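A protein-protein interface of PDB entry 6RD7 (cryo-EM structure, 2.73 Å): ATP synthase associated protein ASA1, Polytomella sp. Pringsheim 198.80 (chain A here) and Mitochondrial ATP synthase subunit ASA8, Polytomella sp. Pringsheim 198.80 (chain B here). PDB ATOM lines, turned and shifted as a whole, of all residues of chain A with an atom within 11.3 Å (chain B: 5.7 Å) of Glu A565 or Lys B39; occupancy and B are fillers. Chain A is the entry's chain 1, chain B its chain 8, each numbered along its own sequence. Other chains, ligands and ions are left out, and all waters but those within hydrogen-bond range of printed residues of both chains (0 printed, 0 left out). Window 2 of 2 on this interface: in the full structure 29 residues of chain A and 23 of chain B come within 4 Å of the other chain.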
ATOM      1  N   LYS A 555      12.701 -32.372  23.002  1.00  0.00           N
ATOM      2  CA  LYS A 555      13.764 -32.743  23.934  1.00  0.00           C
ATOM      3  C   LYS A 555      15.123 -32.210  23.487  1.00  0.00           C
ATOM      4  O   LYS A 555      15.923 -31.759  24.320  1.00  0.00           O
ATOM      5  CB  LYS A 555      13.808 -34.255  24.090  1.00  0.00           C
ATOM      6  CG  LYS A 555      12.620 -34.821  24.814  1.00  0.00           C
ATOM      7  CD  LYS A 555      12.498 -36.296  24.560  1.00  0.00           C
ATOM      8  CE  LYS A 555      11.173 -36.807  25.032  1.00  0.00           C
ATOM      9  NZ  LYS A 555      11.245 -38.238  25.386  1.00  0.00           N
ATOM     10  N   ILE A 556      15.401 -32.244  22.182  1.00  0.00           N
ATOM     11  CA  ILE A 556      16.648 -31.683  21.664  1.00  0.00           C
ATOM     12  C   ILE A 556      16.666 -30.169  21.849  1.00  0.00           C
ATOM     13  O   ILE A 556      17.703 -29.575  22.176  1.00  0.00           O
ATOM     14  CB  ILE A 556      16.833 -32.095  20.190  1.00  0.00           C
ATOM     15  CG1 ILE A 556      17.058 -33.598  20.086  1.00  0.00           C
ATOM     16  CG2 ILE A 556      18.014 -31.408  19.557  1.00  0.00           C
ATOM     17  CD1 ILE A 556      16.833 -34.132  18.710  1.00  0.00           C
ATOM     18  N   ASP A 557      15.507 -29.528  21.703  1.00  0.00           N
ATOM     19  CA  ASP A 557      15.410 -28.096  21.940  1.00  0.00           C
ATOM     20  C   ASP A 557      15.566 -27.768  23.416  1.00  0.00           C
ATOM     21  O   ASP A 557      16.072 -26.698  23.763  1.00  0.00           O
ATOM     22  CB  ASP A 557      14.078 -27.571  21.413  1.00  0.00           C
ATOM     23  CG  ASP A 557      14.067 -27.412  19.910  1.00  0.00           C
ATOM     24  OD1 ASP A 557      15.118 -27.638  19.278  1.00  0.00           O
ATOM     25  OD2 ASP A 557      13.006 -27.066  19.357  1.00  0.00           O
ATOM     26  N   TRP A 558      15.126 -28.667  24.301  1.00  0.00           N
ATOM     27  CA  TRP A 558      15.397 -28.485  25.724  1.00  0.00           C
ATOM     28  C   TRP A 558      16.885 -28.562  26.007  1.00  0.00           C
ATOM     29  O   TRP A 558      17.400 -27.820  26.848  1.00  0.00           O
ATOM     30  CB  TRP A 558      14.660 -29.530  26.563  1.00  0.00           C
ATOM     31  CG  TRP A 558      14.823 -29.308  28.050  1.00  0.00           C
ATOM     32  CD1 TRP A 558      14.000 -28.588  28.854  1.00  0.00           C
ATOM     33  CD2 TRP A 558      15.880 -29.794  28.896  1.00  0.00           C
ATOM     34  NE1 TRP A 558      14.468 -28.594  30.140  1.00  0.00           N
ATOM     35  CE2 TRP A 558      15.622 -29.327  30.192  1.00  0.00           C
ATOM     36  CE3 TRP A 558      17.019 -30.574  28.678  1.00  0.00           C
ATOM     37  CZ2 TRP A 558      16.454 -29.612  31.262  1.00  0.00           C
ATOM     38  CZ3 TRP A 558      17.840 -30.855  29.739  1.00  0.00           C
ATOM     39  CH2 TRP A 558      17.556 -30.379  31.016  1.00  0.00           C
ATOM     40  N   GLU A 559      17.578 -29.494  25.350  1.00  0.00           N
ATOM     41  CA  GLU A 559      19.021 -29.619  25.531  1.00  0.00           C
ATOM     42  C   GLU A 559      19.755 -28.377  25.048  1.00  0.00           C
ATOM     43  O   GLU A 559      20.694 -27.913  25.700  1.00  0.00           O
ATOM     44  CB  GLU A 559      19.540 -30.843  24.790  1.00  0.00           C
ATOM     45  CG  GLU A 559      19.718 -32.051  25.652  1.00  0.00           C
ATOM     46  CD  GLU A 559      20.204 -33.244  24.869  1.00  0.00           C
ATOM     47  OE1 GLU A 559      21.420 -33.513  24.887  1.00  0.00           O
ATOM     48  OE2 GLU A 559      19.374 -33.909  24.223  1.00  0.00           O
ATOM     49  N   THR A 560      19.343 -27.832  23.904  1.00  0.00           N
ATOM     50  CA  THR A 560      19.974 -26.621  23.387  1.00  0.00           C
ATOM     51  C   THR A 560      19.648 -25.414  24.259  1.00  0.00           C
ATOM     52  O   THR A 560      20.504 -24.553  24.485  1.00  0.00           O
ATOM     53  CB  THR A 560      19.536 -26.390  21.941  1.00  0.00           C
ATOM     54  OG1 THR A 560      19.827 -27.556  21.166  1.00  0.00           O
ATOM     55  CG2 THR A 560      20.257 -25.211  21.325  1.00  0.00           C
ATOM     56  N   THR A 561      18.425 -25.357  24.790  1.00  0.00           N
ATOM     57  CA  THR A 561      18.006 -24.224  25.608  1.00  0.00           C
ATOM     58  C   THR A 561      18.727 -24.201  26.948  1.00  0.00           C
ATOM     59  O   THR A 561      19.060 -23.130  27.465  1.00  0.00           O
ATOM     60  CB  THR A 561      16.494 -24.274  25.824  1.00  0.00           C
ATOM     61  OG1 THR A 561      15.847 -24.591  24.590  1.00  0.00           O
ATOM     62  CG2 THR A 561      15.975 -22.950  26.306  1.00  0.00           C
ATOM     63  N   ASN A 562      18.990 -25.371  27.520  1.00  0.00           N
ATOM     64  CA  ASN A 562      19.575 -25.471  28.847  1.00  0.00           C
ATOM     65  C   ASN A 562      21.084 -25.630  28.816  1.00  0.00           C
ATOM     66  O   ASN A 562      21.647 -26.189  29.763  1.00  0.00           O
ATOM     67  CB  ASN A 562      18.937 -26.627  29.611  1.00  0.00           C
ATOM     68  CG  ASN A 562      17.541 -26.304  30.068  1.00  0.00           C
ATOM     69  OD1 ASN A 562      16.591 -26.394  29.301  1.00  0.00           O
ATOM     70  ND2 ASN A 562      17.410 -25.907  31.323  1.00  0.00           N
ATOM     71  N   ALA A 563      21.731 -25.161  27.742  1.00  0.00           N
ATOM     72  CA  ALA A 563      23.191 -25.118  27.584  1.00  0.00           C
ATOM     73  C   ALA A 563      23.821 -26.503  27.686  1.00  0.00           C
ATOM     74  O   ALA A 563      24.946 -26.666  28.156  1.00  0.00           O
ATOM     75  CB  ALA A 563      23.832 -24.148  28.577  1.00  0.00           C
ATOM     76  N   LEU A 564      23.083 -27.510  27.238  1.00  0.00           N
ATOM     77  CA  LEU A 564      23.556 -28.886  27.204  1.00  0.00           C
ATOM     78  C   LEU A 564      23.619 -29.397  25.775  1.00  0.00           C
ATOM     79  O   LEU A 564      23.324 -30.561  25.516  1.00  0.00           O
ATOM     80  CB  LEU A 564      22.664 -29.791  28.047  1.00  0.00           C
ATOM     81  CG  LEU A 564      22.701 -29.582  29.554  1.00  0.00           C
ATOM     82  CD1 LEU A 564      21.464 -30.179  30.178  1.00  0.00           C
ATOM     83  CD2 LEU A 564      23.949 -30.202  30.136  1.00  0.00           C
ATOM     84  N   GLU A 565      23.986 -28.526  24.834  1.00  0.00           N
ATOM     85  CA  GLU A 565      24.048 -28.934  23.440  1.00  0.00           C
ATOM     86  C   GLU A 565      25.206 -29.885  23.173  1.00  0.00           C
ATOM     87  O   GLU A 565      25.142 -30.673  22.228  1.00  0.00           O
ATOM     88  CB  GLU A 565      24.134 -27.706  22.536  1.00  0.00           C
ATOM     89  CG  GLU A 565      25.412 -26.912  22.666  1.00  0.00           C
ATOM     90  CD  GLU A 565      25.276 -25.758  23.628  1.00  0.00           C
ATOM     91  OE1 GLU A 565      24.214 -25.640  24.268  1.00  0.00           O
ATOM     92  OE2 GLU A 565      26.232 -24.969  23.750  1.00  0.00           O
ATOM     93  N   ASP A 566      26.235 -29.869  24.012  1.00  0.00           N
ATOM     94  CA  ASP A 566      27.358 -30.781  23.886  1.00  0.00           C
ATOM     95  C   ASP A 566      27.268 -31.933  24.872  1.00  0.00           C
ATOM     96  O   ASP A 566      28.302 -32.429  25.326  1.00  0.00           O
ATOM     97  CB  ASP A 566      28.668 -30.023  24.083  1.00  0.00           C
ATOM     98  CG  ASP A 566      28.715 -29.279  25.408  1.00  0.00           C
ATOM     99  OD1 ASP A 566      27.681 -28.716  25.818  1.00  0.00           O
ATOM    100  OD2 ASP A 566      29.786 -29.257  26.045  1.00  0.00           O
ATOM    101  N   PHE A 567      26.053 -32.370  25.217  1.00  0.00           N
ATOM    102  CA  PHE A 567      25.909 -33.339  26.297  1.00  0.00           C
ATOM    103  C   PHE A 567      26.331 -34.732  25.862  1.00  0.00           C
ATOM    104  O   PHE A 567      26.908 -35.483  26.654  1.00  0.00           O
ATOM    105  CB  PHE A 567      24.477 -33.364  26.820  1.00  0.00           C
ATOM    106  CG  PHE A 567      24.306 -34.228  28.025  1.00  0.00           C
ATOM    107  CD1 PHE A 567      24.957 -33.917  29.205  1.00  0.00           C
ATOM    108  CD2 PHE A 567      23.523 -35.366  27.976  1.00  0.00           C
ATOM    109  CE1 PHE A 567      24.819 -34.713  30.317  1.00  0.00           C
ATOM    110  CE2 PHE A 567      23.381 -36.167  29.089  1.00  0.00           C
ATOM    111  CZ  PHE A 567      24.034 -35.840  30.259  1.00  0.00           C
ATOM    112  N   ASP A 568      26.060 -35.101  24.610  1.00  0.00           N
ATOM    113  CA  ASP A 568      26.558 -36.381  24.119  1.00  0.00           C
ATOM    114  C   ASP A 568      28.066 -36.339  23.914  1.00  0.00           C
ATOM    115  O   ASP A 568      28.743 -37.357  24.089  1.00  0.00           O
ATOM    116  CB  ASP A 568      25.832 -36.779  22.836  1.00  0.00           C
ATOM    117  CG  ASP A 568      26.182 -35.895  21.663  1.00  0.00           C
ATOM    118  OD1 ASP A 568      25.922 -34.679  21.735  1.00  0.00           O
ATOM    119  OD2 ASP A 568      26.712 -36.419  20.664  1.00  0.00           O
ATOM    120  N   ILE A 569      28.613 -35.163  23.604  1.00  0.00           N
ATOM    121  CA  ILE A 569      30.062 -34.995  23.570  1.00  0.00           C
ATOM    122  C   ILE A 569      30.640 -35.103  24.976  1.00  0.00           C
ATOM    123  O   ILE A 569      31.722 -35.664  25.174  1.00  0.00           O
ATOM    124  CB  ILE A 569      30.421 -33.655  22.902  1.00  0.00           C
ATOM    125  CG1 ILE A 569      29.745 -33.544  21.539  1.00  0.00           C
ATOM    126  CG2 ILE A 569      31.919 -33.510  22.737  1.00  0.00           C
ATOM    127  CD1 ILE A 569      29.998 -32.234  20.843  1.00  0.00           C
ATOM    128  N   THR A 570      29.914 -34.589  25.972  1.00  0.00           N
ATOM    129  CA  THR A 570      30.345 -34.699  27.362  1.00  0.00           C
ATOM    130  C   THR A 570      30.327 -36.149  27.834  1.00  0.00           C
ATOM    131  O   THR A 570      31.251 -36.598  28.520  1.00  0.00           O
ATOM    132  CB  THR A 570      29.450 -33.820  28.240  1.00  0.00           C
ATOM    133  OG1 THR A 570      29.617 -32.451  27.863  1.00  0.00           O
ATOM    134  CG2 THR A 570      29.792 -33.960  29.709  1.00  0.00           C
ATOM    135  N   LEU A 571      29.304 -36.908  27.441  1.00  0.00           N
ATOM    136  CA  LEU A 571      29.262 -38.325  27.782  1.00  0.00           C
ATOM    137  C   LEU A 571      30.304 -39.125  27.011  1.00  0.00           C
ATOM    138  O   LEU A 571      30.750 -40.172  27.485  1.00  0.00           O
ATOM    139  CB  LEU A 571      27.869 -38.890  27.520  1.00  0.00           C
ATOM    140  CG  LEU A 571      26.721 -38.324  28.352  1.00  0.00           C
ATOM    141  CD1 LEU A 571      25.408 -38.876  27.853  1.00  0.00           C
ATOM    142  CD2 LEU A 571      26.910 -38.622  29.820  1.00  0.00           C
ATOM    143  N   ASP A 572      30.696 -38.659  25.825  1.00  0.00           N
ATOM    144  CA  ASP A 572      31.817 -39.271  25.122  1.00  0.00           C
ATOM    145  C   ASP A 572      33.144 -38.962  25.804  1.00  0.00           C
ATOM    146  O   ASP A 572      34.069 -39.779  25.758  1.00  0.00           O
ATOM    147  CB  ASP A 572      31.856 -38.789  23.675  1.00  0.00           C
ATOM    148  CG  ASP A 572      30.899 -39.542  22.787  1.00  0.00           C
ATOM    149  OD1 ASP A 572      30.383 -40.590  23.222  1.00  0.00           O
ATOM    150  OD2 ASP A 572      30.662 -39.087  21.648  1.00  0.00           O
ATOM    151  N   ASP A 573      33.256 -37.783  26.419  1.00  0.00           N
ATOM    152  CA  ASP A 573      34.500 -37.394  27.075  1.00  0.00           C
ATOM    153  C   ASP A 573      34.737 -38.208  28.337  1.00  0.00           C
ATOM    154  O   ASP A 573      35.876 -38.574  28.646  1.00  0.00           O
ATOM    155  CB  ASP A 573      34.474 -35.904  27.412  1.00  0.00           C
ATOM    156  CG  ASP A 573      34.614 -35.028  26.193  1.00  0.00           C
ATOM    157  OD1 ASP A 573      35.119 -35.517  25.163  1.00  0.00           O
ATOM    158  OD2 ASP A 573      34.218 -33.847  26.262  1.00  0.00           O
ATOM    159  N   LYS A 580      25.349 -42.765  27.762  1.00  0.00           N
ATOM    160  CA  LYS A 580      25.010 -42.315  26.415  1.00  0.00           C
ATOM    161  C   LYS A 580      23.911 -43.180  25.811  1.00  0.00           C
ATOM    162  O   LYS A 580      23.019 -42.676  25.114  1.00  0.00           O
ATOM    163  CB  LYS A 580      26.255 -42.333  25.535  1.00  0.00           C
ATOM    164  CG  LYS A 580      26.057 -41.749  24.157  1.00  0.00           C
ATOM    165  CD  LYS A 580      27.330 -41.867  23.352  1.00  0.00           C
ATOM    166  CE  LYS A 580      27.110 -41.504  21.898  1.00  0.00           C
ATOM    167  NZ  LYS A 580      26.771 -40.070  21.721  1.00  0.00           N
ATOM    168  N   TRP A 583      20.844 -41.984  27.465  1.00  0.00           N
ATOM    169  CA  TRP A 583      20.450 -40.685  26.926  1.00  0.00           C
ATOM    170  C   TRP A 583      19.708 -40.839  25.608  1.00  0.00           C
ATOM    171  O   TRP A 583      18.650 -40.223  25.401  1.00  0.00           O
ATOM    172  CB  TRP A 583      21.699 -39.823  26.751  1.00  0.00           C
ATOM    173  CG  TRP A 583      21.574 -38.651  25.837  1.00  0.00           C
ATOM    174  CD1 TRP A 583      21.100 -37.418  26.153  1.00  0.00           C
ATOM    175  CD2 TRP A 583      21.977 -38.587  24.468  1.00  0.00           C
ATOM    176  NE1 TRP A 583      21.162 -36.594  25.062  1.00  0.00           N
ATOM    177  CE2 TRP A 583      21.697 -37.289  24.012  1.00  0.00           C
ATOM    178  CE3 TRP A 583      22.536 -39.507  23.578  1.00  0.00           C
ATOM    179  CZ2 TRP A 583      21.959 -36.885  22.711  1.00  0.00           C
ATOM    180  CZ3 TRP A 583      22.792 -39.106  22.289  1.00  0.00           C
ATOM    181  CH2 TRP A 583      22.508 -37.807  21.866  1.00  0.00           C
ATOM    182  N   ASN A 587      15.643 -40.131  25.089  1.00  0.00           N
ATOM    183  CA  ASN A 587      15.167 -39.131  24.142  1.00  0.00           C
ATOM    184  C   ASN A 587      14.170 -39.725  23.158  1.00  0.00           C
ATOM    185  O   ASN A 587      13.398 -38.994  22.531  1.00  0.00           O
ATOM    186  CB  ASN A 587      16.333 -38.500  23.400  1.00  0.00           C
ATOM    187  CG  ASN A 587      17.041 -37.454  24.219  1.00  0.00           C
ATOM    188  OD1 ASN A 587      16.432 -36.768  25.033  1.00  0.00           O
ATOM    189  ND2 ASN A 587      18.335 -37.313  23.998  1.00  0.00           N
ATOM    190  N   PHE B  28      14.787 -19.905  21.193  1.00  0.00           N
ATOM    191  CA  PHE B  28      15.715 -18.797  21.008  1.00  0.00           C
ATOM    192  C   PHE B  28      15.419 -18.052  19.716  1.00  0.00           C
ATOM    193  O   PHE B  28      15.639 -16.841  19.624  1.00  0.00           O
ATOM    194  CB  PHE B  28      17.157 -19.302  21.001  1.00  0.00           C
ATOM    195  CG  PHE B  28      17.648 -19.804  22.331  1.00  0.00           C
ATOM    196  CD1 PHE B  28      16.976 -19.515  23.502  1.00  0.00           C
ATOM    197  CD2 PHE B  28      18.797 -20.563  22.399  1.00  0.00           C
ATOM    198  CE1 PHE B  28      17.437 -19.975  24.708  1.00  0.00           C
ATOM    199  CE2 PHE B  28      19.257 -21.027  23.602  1.00  0.00           C
ATOM    200  CZ  PHE B  28      18.578 -20.728  24.757  1.00  0.00           C
ATOM    201  N   THR B  34      14.177 -14.624  25.695  1.00  0.00           N
ATOM    202  CA  THR B  34      14.421 -15.971  26.196  1.00  0.00           C
ATOM    203  C   THR B  34      15.885 -16.353  26.039  1.00  0.00           C
ATOM    204  O   THR B  34      16.489 -16.921  26.957  1.00  0.00           O
ATOM    205  CB  THR B  34      13.515 -16.958  25.461  1.00  0.00           C
ATOM    206  OG1 THR B  34      12.150 -16.659  25.763  1.00  0.00           O
ATOM    207  CG2 THR B  34      13.802 -18.389  25.864  1.00  0.00           C
ATOM    208  N   TYR B  35      16.484 -16.000  24.902  1.00  0.00           N
ATOM    209  CA  TYR B  35      17.901 -16.262  24.687  1.00  0.00           C
ATOM    210  C   TYR B  35      18.769 -15.418  25.606  1.00  0.00           C
ATOM    211  O   TYR B  35      19.810 -15.882  26.084  1.00  0.00           O
ATOM    212  CB  TYR B  35      18.260 -15.998  23.229  1.00  0.00           C
ATOM    213  CG  TYR B  35      19.739 -15.999  22.980  1.00  0.00           C
ATOM    214  CD1 TYR B  35      20.485 -17.149  23.176  1.00  0.00           C
ATOM    215  CD2 TYR B  35      20.396 -14.851  22.564  1.00  0.00           C
ATOM    216  CE1 TYR B  35      21.832 -17.159  22.963  1.00  0.00           C
ATOM    217  CE2 TYR B  35      21.751 -14.853  22.344  1.00  0.00           C
ATOM    218  CZ  TYR B  35      22.463 -16.014  22.544  1.00  0.00           C
ATOM    219  OH  TYR B  35      23.815 -16.031  22.329  1.00  0.00           O
ATOM    220  N   ALA B  36      18.353 -14.181  25.871  1.00  0.00           N
ATOM    221  CA  ALA B  36      19.144 -13.293  26.710  1.00  0.00           C
ATOM    222  C   ALA B  36      19.116 -13.742  28.162  1.00  0.00           C
ATOM    223  O   ALA B  36      20.147 -13.758  28.836  1.00  0.00           O
ATOM    224  CB  ALA B  36      18.641 -11.859  26.576  1.00  0.00           C
ATOM    225  N   THR B  37      17.947 -14.143  28.653  1.00  0.00           N
ATOM    226  CA  THR B  37      17.832 -14.482  30.064  1.00  0.00           C
ATOM    227  C   THR B  37      18.234 -15.925  30.331  1.00  0.00           C
ATOM    228  O   THR B  37      18.575 -16.279  31.464  1.00  0.00           O
ATOM    229  CB  THR B  37      16.408 -14.226  30.547  1.00  0.00           C
ATOM    230  OG1 THR B  37      15.481 -14.705  29.568  1.00  0.00           O
ATOM    231  CG2 THR B  37      16.193 -12.747  30.755  1.00  0.00           C
ATOM    232  N   LYS B  38      18.204 -16.779  29.308  1.00  0.00           N
ATOM    233  CA  LYS B  38      18.424 -18.199  29.563  1.00  0.00           C
ATOM    234  C   LYS B  38      19.796 -18.662  29.095  1.00  0.00           C
ATOM    235  O   LYS B  38      20.354 -19.607  29.662  1.00  0.00           O
ATOM    236  CB  LYS B  38      17.320 -19.027  28.913  1.00  0.00           C
ATOM    237  CG  LYS B  38      16.007 -18.968  29.671  1.00  0.00           C
ATOM    238  CD  LYS B  38      14.973 -19.901  29.084  1.00  0.00           C
ATOM    239  CE  LYS B  38      15.203 -21.327  29.540  1.00  0.00           C
ATOM    240  NZ  LYS B  38      14.893 -21.524  30.978  1.00  0.00           N
ATOM    241  N   LYS B  39      20.362 -18.035  28.067  1.00  0.00           N
ATOM    242  CA  LYS B  39      21.678 -18.462  27.605  1.00  0.00           C
ATOM    243  C   LYS B  39      22.686 -17.334  27.478  1.00  0.00           C
ATOM    244  O   LYS B  39      23.858 -17.540  27.795  1.00  0.00           O
ATOM    245  CB  LYS B  39      21.571 -19.201  26.264  1.00  0.00           C
ATOM    246  CG  LYS B  39      22.827 -19.988  25.928  1.00  0.00           C
ATOM    247  CD  LYS B  39      22.673 -20.834  24.700  1.00  0.00           C
ATOM    248  CE  LYS B  39      22.938 -22.284  25.015  1.00  0.00           C
ATOM    249  NZ  LYS B  39      22.668 -23.152  23.844  1.00  0.00           N
ATOM    250  N   LEU B  40      22.278 -16.146  27.027  1.00  0.00           N
ATOM    251  CA  LEU B  40      23.265 -15.121  26.692  1.00  0.00           C
ATOM    252  C   LEU B  40      23.924 -14.546  27.937  1.00  0.00           C
ATOM    253  O   LEU B  40      25.154 -14.526  28.033  1.00  0.00           O
ATOM    254  CB  LEU B  40      22.633 -14.012  25.863  1.00  0.00           C
ATOM    255  CG  LEU B  40      23.557 -12.843  25.538  1.00  0.00           C
ATOM    256  CD1 LEU B  40      24.664 -13.287  24.608  1.00  0.00           C
ATOM    257  CD2 LEU B  40      22.773 -11.705  24.926  1.00  0.00           C
ATOM    258  N   ILE B  41      23.131 -14.111  28.911  1.00  0.00           N
ATOM    259  CA  ILE B  41      23.692 -13.684  30.192  1.00  0.00           C
ATOM    260  C   ILE B  41      24.349 -14.858  30.922  1.00  0.00           C
ATOM    261  O   ILE B  41      25.583 -14.822  31.036  1.00  0.00           O
ATOM    262  CB  ILE B  41      22.650 -12.958  31.064  1.00  0.00           C
ATOM    263  CG1 ILE B  41      22.157 -11.683  30.375  1.00  0.00           C
ATOM    264  CG2 ILE B  41      23.241 -12.619  32.408  1.00  0.00           C
ATOM    265  CD1 ILE B  41      23.250 -10.784  29.868  1.00  0.00           C
ATOM    266  N   PRO B  42      23.651 -15.942  31.337  1.00  0.00           N
ATOM    267  CA  PRO B  42      24.283 -16.874  32.291  1.00  0.00           C
ATOM    268  C   PRO B  42      25.400 -17.727  31.713  1.00  0.00           C
ATOM    269  O   PRO B  42      26.134 -18.360  32.480  1.00  0.00           O
ATOM    270  CB  PRO B  42      23.111 -17.755  32.746  1.00  0.00           C
ATOM    271  CG  PRO B  42      21.895 -17.157  32.155  1.00  0.00           C
ATOM    272  CD  PRO B  42      22.358 -16.516  30.920  1.00  0.00           C
ATOM    273  N   ARG B  43      25.559 -17.771  30.398  1.00  0.00           N
ATOM    274  CA  ARG B  43      26.660 -18.508  29.804  1.00  0.00           C
ATOM    275  C   ARG B  43      27.665 -17.635  29.075  1.00  0.00           C
ATOM    276  O   ARG B  43      28.829 -18.024  28.984  1.00  0.00           O
ATOM    277  CB  ARG B  43      26.141 -19.575  28.830  1.00  0.00           C
ATOM    278  CG  ARG B  43      25.220 -20.597  29.457  1.00  0.00           C
ATOM    279  CD  ARG B  43      25.988 -21.569  30.318  1.00  0.00           C
ATOM    280  NE  ARG B  43      26.748 -22.515  29.514  1.00  0.00           N
ATOM    281  CZ  ARG B  43      27.709 -23.293  29.995  1.00  0.00           C
ATOM    282  NH1 ARG B  43      28.025 -23.231  31.276  1.00  0.00           N
ATOM    283  NH2 ARG B  43      28.352 -24.128  29.196  1.00  0.00           N
ATOM    284  N   HIS B  44      27.266 -16.472  28.561  1.00  0.00           N
ATOM    285  CA  HIS B  44      28.139 -15.647  27.741  1.00  0.00           C
ATOM    286  C   HIS B  44      28.401 -14.287  28.373  1.00  0.00           C
ATOM    287  O   HIS B  44      28.863 -13.364  27.690  1.00  0.00           O
ATOM    288  CB  HIS B  44      27.554 -15.463  26.344  1.00  0.00           C
ATOM    289  CG  HIS B  44      27.208 -16.745  25.656  1.00  0.00           C
ATOM    290  ND1 HIS B  44      28.067 -17.817  25.603  1.00  0.00           N
ATOM    291  CD2 HIS B  44      26.096 -17.122  24.987  1.00  0.00           C
ATOM    292  CE1 HIS B  44      27.501 -18.802  24.933  1.00  0.00           C
ATOM    293  NE2 HIS B  44      26.303 -18.406  24.549  1.00  0.00           N
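Of the 22 printed residues of chain A, 4 touch a printed residue of chain B.
Printed residues of chain A that touch a printed residue of chain B: Thr A560, Thr A561, Ala A563 and Glu A565.
Hydrophobic or aromatic side chains of chain A within 4 Å of the printed part of chain B: Ala A563.
Along chain B the printed residues that touch a printed residue of chain A span positions 28 to 43.
Among the printed residues, 7 pairs touch across the chains.
Ile A556 touches none of the printed residues of chain B.
Of the printed residues of chain B, Thr A560 touches Phe B28 and Lys B39.
Of the printed residues of chain B, Thr A561 touches Phe B28 (3.6 Å) and Lys B38 (3.7 Å).
Of the printed residues of chain B, Ala A563 touches Lys B39 and Arg B43.
Asp A568 touches none of the printed residues of chain B.
Of the printed residues of chain A, Phe B28 touches Thr A560 (3.8 Å) and Thr A561 (3.6 Å).
Of chain A, only Thr A561 comes within 4 Å of Lys B38.
Of chain A, only Thr A560 (2.7 Å), Ala A563 (3.8 Å) and Glu A565 (3.0 Å) come within 4 Å of Lys B39.
No residue of chain A comes within 4 Å of Leu B40.
No residue of chain A comes within 4 Å of Ile B41.
No residue of chain A comes within 4 Å of Pro B42.
Printed residues of chain A within 4 Å of Arg B43: Ala A563.
No residue of chain A comes within 4 Å of His B44.
The nearest residue of chain A that does not touch Lys B39 is Thr A561 (4.7 Å).
The nearest printed residue of chain A that does not touch Phe B28 is Asn A562 (5.4 Å).
Thr A560 touches Phe B28.
Thr A561 touches Phe B28.
CE of Lys B38 touches CG2 of Thr A561, 3.7 Å away.
Lys B39 touches Ala A563.
Arg B43 touches Ala A563.
The backbone carbonyl oxygen (O) of Ile A556 is in hydrogen-bond range of the side-chain hydroxyl (OG1) of Thr A560 (3.1 Å).
O of Glu A559 is in hydrogen-bond range of N of Glu A565 (3.5 Å).
NZ of Lys B39 sits at hydrogen-bond distance from O of Thr A560, 2.7 Å away.
The side-chain carboxylate (OE1) of Glu A565 is in salt-bridge range of the side-chain amino group (NZ) of Lys B39 (3.0 Å).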
